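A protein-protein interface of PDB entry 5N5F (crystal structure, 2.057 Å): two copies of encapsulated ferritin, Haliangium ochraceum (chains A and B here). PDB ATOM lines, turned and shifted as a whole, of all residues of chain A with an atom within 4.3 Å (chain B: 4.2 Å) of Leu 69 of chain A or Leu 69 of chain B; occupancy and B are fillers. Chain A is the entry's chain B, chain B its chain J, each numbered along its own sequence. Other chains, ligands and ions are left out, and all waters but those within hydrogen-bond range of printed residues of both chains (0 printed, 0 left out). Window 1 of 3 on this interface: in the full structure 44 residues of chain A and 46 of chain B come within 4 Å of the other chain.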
ATOM      1  N   LEU A  28      16.823   1.810  25.589  1.00  0.00           N
ATOM      2  CA  LEU A  28      16.000   0.744  25.030  1.00  0.00           C
ATOM      3  C   LEU A  28      15.761  -0.349  26.063  1.00  0.00           C
ATOM      4  O   LEU A  28      14.634  -0.830  26.223  1.00  0.00           O
ATOM      5  CB  LEU A  28      16.665   0.173  23.775  1.00  0.00           C
ATOM      6  CG  LEU A  28      16.013  -1.057  23.138  1.00  0.00           C
ATOM      7  CD1 LEU A  28      14.530  -0.827  22.876  1.00  0.00           C
ATOM      8  CD2 LEU A  28      16.726  -1.424  21.846  1.00  0.00           C
ATOM      9  N   ALA A  65      10.598   2.475  22.856  1.00  0.00           N
ATOM     10  CA  ALA A  65      11.613   1.478  22.535  1.00  0.00           C
ATOM     11  C   ALA A  65      11.896   1.435  21.039  1.00  0.00           C
ATOM     12  O   ALA A  65      13.056   1.367  20.619  1.00  0.00           O
ATOM     13  CB  ALA A  65      11.162   0.105  23.029  1.00  0.00           C
ATOM     14  N   MET A  66      10.844   1.468  20.217  1.00  0.00           N
ATOM     15  CA  MET A  66      11.029   1.368  18.774  1.00  0.00           C
ATOM     16  C   MET A  66      11.570   2.665  18.183  1.00  0.00           C
ATOM     17  O   MET A  66      12.260   2.633  17.157  1.00  0.00           O
ATOM     18  CB  MET A  66       9.712   0.975  18.108  1.00  0.00           C
ATOM     19  CG  MET A  66       9.172  -0.379  18.570  1.00  0.00           C
ATOM     20  SD  MET A  66      10.309  -1.763  18.288  1.00  0.00           S
ATOM     21  CE  MET A  66      11.161  -1.872  19.862  1.00  0.00           C
ATOM     22  N   MET A  67      11.277   3.807  18.809  1.00  0.00           N
ATOM     23  CA  MET A  67      11.943   5.048  18.429  1.00  0.00           C
ATOM     24  C   MET A  67      13.440   4.949  18.681  1.00  0.00           C
ATOM     25  O   MET A  67      14.256   5.278  17.810  1.00  0.00           O
ATOM     26  CB  MET A  67      11.355   6.228  19.203  1.00  0.00           C
ATOM     27  CG  MET A  67       9.952   6.628  18.779  1.00  0.00           C
ATOM     28  SD  MET A  67       9.149   7.754  19.947  1.00  0.00           S
ATOM     29  CE  MET A  67      10.261   9.151  19.885  1.00  0.00           C
ATOM     30  N   THR A  68      13.819   4.490  19.878  1.00  0.00           N
ATOM     31  CA  THR A  68      15.231   4.332  20.204  1.00  0.00           C
ATOM     32  C   THR A  68      15.895   3.312  19.287  1.00  0.00           C
ATOM     33  O   THR A  68      17.030   3.512  18.840  1.00  0.00           O
ATOM     34  CB  THR A  68      15.384   3.908  21.665  1.00  0.00           C
ATOM     35  OG1 THR A  68      14.706   4.844  22.522  1.00  0.00           O
ATOM     36  CG2 THR A  68      16.851   3.844  22.050  1.00  0.00           C
ATOM     37  N   LEU A  69      15.207   2.205  19.001  1.00  0.00           N
ATOM     38  CA  LEU A  69      15.799   1.163  18.171  1.00  0.00           C
ATOM     39  C   LEU A  69      16.069   1.679  16.765  1.00  0.00           C
ATOM     40  O   LEU A  69      17.104   1.363  16.168  1.00  0.00           O
ATOM     41  CB  LEU A  69      14.886  -0.063  18.137  1.00  0.00           C
ATOM     42  CG  LEU A  69      15.347  -1.257  17.292  1.00  0.00           C
ATOM     43  CD1 LEU A  69      16.735  -1.762  17.702  1.00  0.00           C
ATOM     44  CD2 LEU A  69      14.329  -2.382  17.392  1.00  0.00           C
ATOM     45  N   GLU A  70      15.157   2.491  16.223  1.00  0.00           N
ATOM     46  CA  GLU A  70      15.381   3.073  14.906  1.00  0.00           C
ATOM     47  C   GLU A  70      16.598   3.988  14.911  1.00  0.00           C
ATOM     48  O   GLU A  70      17.351   4.035  13.931  1.00  0.00           O
ATOM     49  CB  GLU A  70      14.137   3.830  14.442  1.00  0.00           C
ATOM     50  CG  GLU A  70      14.305   4.584  13.117  1.00  0.00           C
ATOM     51  CD  GLU A  70      14.618   3.677  11.939  1.00  0.00           C
ATOM     52  OE1 GLU A  70      14.611   2.440  12.111  1.00  0.00           O
ATOM     53  OE2 GLU A  70      14.873   4.206  10.833  1.00  0.00           O
ATOM     54  N   TRP A  71      16.809   4.731  15.999  1.00  0.00           N
ATOM     55  CA  TRP A  71      18.021   5.536  16.095  1.00  0.00           C
ATOM     56  C   TRP A  71      19.260   4.648  16.066  1.00  0.00           C
ATOM     57  O   TRP A  71      20.231   4.943  15.361  1.00  0.00           O
ATOM     58  CB  TRP A  71      17.999   6.384  17.362  1.00  0.00           C
ATOM     59  CG  TRP A  71      19.155   7.327  17.450  1.00  0.00           C
ATOM     60  CD1 TRP A  71      19.167   8.641  17.087  1.00  0.00           C
ATOM     61  CD2 TRP A  71      20.474   7.029  17.924  1.00  0.00           C
ATOM     62  NE1 TRP A  71      20.410   9.182  17.309  1.00  0.00           N
ATOM     63  CE2 TRP A  71      21.232   8.211  17.818  1.00  0.00           C
ATOM     64  CE3 TRP A  71      21.088   5.877  18.428  1.00  0.00           C
ATOM     65  CZ2 TRP A  71      22.570   8.276  18.201  1.00  0.00           C
ATOM     66  CZ3 TRP A  71      22.416   5.943  18.804  1.00  0.00           C
ATOM     67  CH2 TRP A  71      23.142   7.135  18.689  1.00  0.00           C
ATOM     68  N   ILE A  72      19.234   3.547  16.820  1.00  0.00           N
ATOM     69  CA  ILE A  72      20.343   2.599  16.800  1.00  0.00           C
ATOM     70  C   ILE A  72      20.557   2.057  15.391  1.00  0.00           C
ATOM     71  O   ILE A  72      21.695   1.954  14.917  1.00  0.00           O
ATOM     72  CB  ILE A  72      20.084   1.467  17.811  1.00  0.00           C
ATOM     73  CG1 ILE A  72      20.106   2.025  19.236  1.00  0.00           C
ATOM     74  CG2 ILE A  72      21.108   0.343  17.655  1.00  0.00           C
ATOM     75  CD1 ILE A  72      19.675   1.038  20.283  1.00  0.00           C
ATOM     76  N   ARG A  73      19.471   1.698  14.702  1.00  0.00           N
ATOM     77  CA  ARG A  73      19.606   1.068  13.391  1.00  0.00           C
ATOM     78  C   ARG A  73      20.280   1.998  12.393  1.00  0.00           C
ATOM     79  O   ARG A  73      21.047   1.548  11.533  1.00  0.00           O
ATOM     80  CB  ARG A  73      18.240   0.639  12.859  1.00  0.00           C
ATOM     81  CG  ARG A  73      18.320  -0.172  11.562  1.00  0.00           C
ATOM     82  CD  ARG A  73      17.002  -0.169  10.810  1.00  0.00           C
ATOM     83  NE  ARG A  73      16.693   1.150  10.269  1.00  0.00           N
ATOM     84  CZ  ARG A  73      17.125   1.607   9.096  1.00  0.00           C
ATOM     85  NH1 ARG A  73      17.897   0.858   8.322  1.00  0.00           N
ATOM     86  NH2 ARG A  73      16.786   2.825   8.699  1.00  0.00           N
ATOM     87  N   PHE A  79      23.087  -3.859  13.412  1.00  0.00           N
ATOM     88  CA  PHE A  79      21.656  -3.830  13.712  1.00  0.00           C
ATOM     89  C   PHE A  79      20.835  -3.732  12.432  1.00  0.00           C
ATOM     90  O   PHE A  79      19.803  -4.397  12.292  1.00  0.00           O
ATOM     91  CB  PHE A  79      21.326  -2.666  14.647  1.00  0.00           C
ATOM     92  CG  PHE A  79      21.305  -3.040  16.107  1.00  0.00           C
ATOM     93  CD1 PHE A  79      22.471  -3.042  16.856  1.00  0.00           C
ATOM     94  CD2 PHE A  79      20.113  -3.376  16.733  1.00  0.00           C
ATOM     95  CE1 PHE A  79      22.454  -3.381  18.198  1.00  0.00           C
ATOM     96  CE2 PHE A  79      20.087  -3.716  18.079  1.00  0.00           C
ATOM     97  CZ  PHE A  79      21.259  -3.717  18.811  1.00  0.00           C
ATOM     98  N   MET A  83      18.321  -6.718  11.429  1.00  0.00           N
ATOM     99  CA  MET A  83      16.920  -6.305  11.378  1.00  0.00           C
ATOM    100  C   MET A  83      16.326  -6.564   9.997  1.00  0.00           C
ATOM    101  O   MET A  83      15.182  -7.021   9.878  1.00  0.00           O
ATOM    102  CB  MET A  83      16.793  -4.829  11.751  1.00  0.00           C
ATOM    103  CG  MET A  83      17.005  -4.549  13.241  1.00  0.00           C
ATOM    104  SD  MET A  83      17.187  -2.795  13.597  1.00  0.00           S
ATOM    105  CE  MET A  83      15.494  -2.234  13.453  1.00  0.00           C
ATOM    106  N   ALA B  65      19.133 -11.028  19.372  1.00  0.00           N
ATOM    107  CA  ALA B  65      18.166 -10.042  19.844  1.00  0.00           C
ATOM    108  C   ALA B  65      17.086  -9.795  18.799  1.00  0.00           C
ATOM    109  O   ALA B  65      15.894  -9.749  19.122  1.00  0.00           O
ATOM    110  CB  ALA B  65      18.884  -8.740  20.203  1.00  0.00           C
ATOM    111  N   MET B  66      17.481  -9.635  17.533  1.00  0.00           N
ATOM    112  CA  MET B  66      16.485  -9.367  16.504  1.00  0.00           C
ATOM    113  C   MET B  66      15.646 -10.605  16.202  1.00  0.00           C
ATOM    114  O   MET B  66      14.488 -10.478  15.791  1.00  0.00           O
ATOM    115  CB  MET B  66      17.158  -8.835  15.239  1.00  0.00           C
ATOM    116  CG  MET B  66      17.865  -7.482  15.418  1.00  0.00           C
ATOM    117  SD  MET B  66      16.848  -6.165  16.148  1.00  0.00           S
ATOM    118  CE  MET B  66      17.202  -6.363  17.895  1.00  0.00           C
ATOM    119  N   MET B  67      16.188 -11.802  16.424  1.00  0.00           N
ATOM    120  CA  MET B  67      15.355 -13.001  16.371  1.00  0.00           C
ATOM    121  C   MET B  67      14.286 -12.963  17.458  1.00  0.00           C
ATOM    122  O   MET B  67      13.104 -13.221  17.200  1.00  0.00           O
ATOM    123  CB  MET B  67      16.224 -14.253  16.515  1.00  0.00           C
ATOM    124  CG  MET B  67      17.155 -14.505  15.339  1.00  0.00           C
ATOM    125  SD  MET B  67      18.475 -15.687  15.714  1.00  0.00           S
ATOM    126  CE  MET B  67      17.534 -17.180  16.011  1.00  0.00           C
ATOM    127  N   THR B  68      14.684 -12.627  18.688  1.00  0.00           N
ATOM    128  CA  THR B  68      13.723 -12.575  19.785  1.00  0.00           C
ATOM    129  C   THR B  68      12.688 -11.487  19.548  1.00  0.00           C
ATOM    130  O   THR B  68      11.505 -11.666  19.859  1.00  0.00           O
ATOM    131  CB  THR B  68      14.451 -12.336  21.107  1.00  0.00           C
ATOM    132  OG1 THR B  68      15.514 -13.287  21.243  1.00  0.00           O
ATOM    133  CG2 THR B  68      13.490 -12.483  22.285  1.00  0.00           C
ATOM    134  N   LEU B  69      13.117 -10.351  18.998  1.00  0.00           N
ATOM    135  CA  LEU B  69      12.194  -9.259  18.734  1.00  0.00           C
ATOM    136  C   LEU B  69      11.168  -9.648  17.680  1.00  0.00           C
ATOM    137  O   LEU B  69       9.988  -9.292  17.796  1.00  0.00           O
ATOM    138  CB  LEU B  69      12.965  -8.018  18.300  1.00  0.00           C
ATOM    139  CG  LEU B  69      12.136  -6.762  18.044  1.00  0.00           C
ATOM    140  CD1 LEU B  69      11.366  -6.332  19.297  1.00  0.00           C
ATOM    141  CD2 LEU B  69      13.038  -5.642  17.565  1.00  0.00           C
ATOM    142  N   GLU B  70      11.597 -10.367  16.639  1.00  0.00           N
ATOM    143  CA  GLU B  70      10.644 -10.833  15.639  1.00  0.00           C
ATOM    144  C   GLU B  70       9.614 -11.759  16.268  1.00  0.00           C
ATOM    145  O   GLU B  70       8.429 -11.712  15.918  1.00  0.00           O
ATOM    146  CB  GLU B  70      11.376 -11.539  14.493  1.00  0.00           C
ATOM    147  CG  GLU B  70      10.459 -12.202  13.464  1.00  0.00           C
ATOM    148  CD  GLU B  70       9.513 -11.224  12.778  1.00  0.00           C
ATOM    149  OE1 GLU B  70       9.638 -10.001  13.001  1.00  0.00           O
ATOM    150  OE2 GLU B  70       8.641 -11.685  12.009  1.00  0.00           O
ATOM    151  N   TRP B  71      10.045 -12.610  17.202  1.00  0.00           N
ATOM    152  CA  TRP B  71       9.101 -13.485  17.886  1.00  0.00           C
ATOM    153  C   TRP B  71       8.091 -12.674  18.688  1.00  0.00           C
ATOM    154  O   TRP B  71       6.913 -13.041  18.766  1.00  0.00           O
ATOM    155  CB  TRP B  71       9.849 -14.459  18.792  1.00  0.00           C
ATOM    156  CG  TRP B  71       8.946 -15.421  19.508  1.00  0.00           C
ATOM    157  CD1 TRP B  71       8.659 -16.704  19.140  1.00  0.00           C
ATOM    158  CD2 TRP B  71       8.209 -15.176  20.714  1.00  0.00           C
ATOM    159  NE1 TRP B  71       7.791 -17.273  20.044  1.00  0.00           N
ATOM    160  CE2 TRP B  71       7.498 -16.354  21.017  1.00  0.00           C
ATOM    161  CE3 TRP B  71       8.082 -14.074  21.567  1.00  0.00           C
ATOM    162  CZ2 TRP B  71       6.673 -16.463  22.138  1.00  0.00           C
ATOM    163  CZ3 TRP B  71       7.260 -14.183  22.680  1.00  0.00           C
ATOM    164  CH2 TRP B  71       6.568 -15.369  22.954  1.00  0.00           C
ATOM    165  N   ILE B  72       8.532 -11.569  19.291  1.00  0.00           N
ATOM    166  CA  ILE B  72       7.621 -10.728  20.063  1.00  0.00           C
ATOM    167  C   ILE B  72       6.641 -10.022  19.135  1.00  0.00           C
ATOM    168  O   ILE B  72       5.428 -10.027  19.370  1.00  0.00           O
ATOM    169  CB  ILE B  72       8.411  -9.723  20.920  1.00  0.00           C
ATOM    170  CG1 ILE B  72       9.207 -10.467  21.997  1.00  0.00           C
ATOM    171  CG2 ILE B  72       7.459  -8.702  21.571  1.00  0.00           C
ATOM    172  CD1 ILE B  72      10.169  -9.595  22.777  1.00  0.00           C
ATOM    173  N   ARG B  73       7.155  -9.401  18.070  1.00  0.00           N
ATOM    174  CA  ARG B  73       6.292  -8.703  17.120  1.00  0.00           C
ATOM    175  C   ARG B  73       5.149  -9.594  16.646  1.00  0.00           C
ATOM    176  O   ARG B  73       4.030  -9.117  16.433  1.00  0.00           O
ATOM    177  CB  ARG B  73       7.108  -8.220  15.920  1.00  0.00           C
ATOM    178  CG  ARG B  73       6.309  -7.367  14.936  1.00  0.00           C
ATOM    179  CD  ARG B  73       6.940  -7.347  13.551  1.00  0.00           C
ATOM    180  NE  ARG B  73       6.970  -8.671  12.935  1.00  0.00           N
ATOM    181  CZ  ARG B  73       5.965  -9.210  12.249  1.00  0.00           C
ATOM    182  NH1 ARG B  73       4.828  -8.545  12.081  1.00  0.00           N
ATOM    183  NH2 ARG B  73       6.095 -10.423  11.728  1.00  0.00           N
ATOM    184  N   PHE B  79       3.670  -3.860  19.459  1.00  0.00           N
ATOM    185  CA  PHE B  79       5.006  -3.864  18.872  1.00  0.00           C
ATOM    186  C   PHE B  79       4.921  -3.748  17.355  1.00  0.00           C
ATOM    187  O   PHE B  79       5.596  -2.914  16.740  1.00  0.00           O
ATOM    188  CB  PHE B  79       5.754  -5.136  19.273  1.00  0.00           C
ATOM    189  CG  PHE B  79       6.565  -5.001  20.533  1.00  0.00           C
ATOM    190  CD1 PHE B  79       7.869  -4.530  20.489  1.00  0.00           C
ATOM    191  CD2 PHE B  79       6.032  -5.362  21.760  1.00  0.00           C
ATOM    192  CE1 PHE B  79       8.623  -4.416  21.644  1.00  0.00           C
ATOM    193  CE2 PHE B  79       6.780  -5.248  22.920  1.00  0.00           C
ATOM    194  CZ  PHE B  79       8.075  -4.772  22.861  1.00  0.00           C
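Among the printed residues, pairs that only touch across the chains: Leu 69 of chain A with Leu 69 of chain B (3.5 Å), Phe 79 of chain A with Met 66 of chain B (3.9 Å) and Met 83 of chain A with Met 66 of chain B (3.3 Å).
Leu 69 of chain A touches one residue of chain B. Of the printed residues of chain B, Phe 79 of chain A touches Met 66. Printed residues of chain B within 4 Å of Met 83 of chain A: Met 66 (3.3 Å). Of chain A, only Leu 69 (3.5 Å) comes within 4 Å of Leu 69 of chain B. The nearest printed residue of chain A that does not touch Leu 69 of chain B is Met 66 of chain A (4.5 Å). The nearest printed residue of chain B that does not touch Phe 79 of chain A is Ala 65 of chain B (5.6 Å).
Of the 12 printed residues of chain A, 3 touch a printed residue of chain B. Printed residues of chain A that touch a printed residue of chain B: Leu 69, Phe 79 and Met 83. Hydrophobic or aromatic side chains of chain A that line the printed part of chain B: Leu 69, Phe 79 and Met 83. Hydrophobic or aromatic side chains of chain B that line the printed part of chain A: Met 66 and Leu 69. Among the printed residues, 3 pairs touch across the chains. Among the printed residues, no Asp or Glu carboxylate lies within 4 Å of a Lys or Arg side-chain nitrogen of the other chain.
Leu 69 of chain A touches its own counterpart, Leu 69 of chain B. Phe 79 of chain A touches Met 66 of chain B, but with the chains exchanged Met 66 of chain A does not touch Phe 79 of chain B (4.01 Å).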
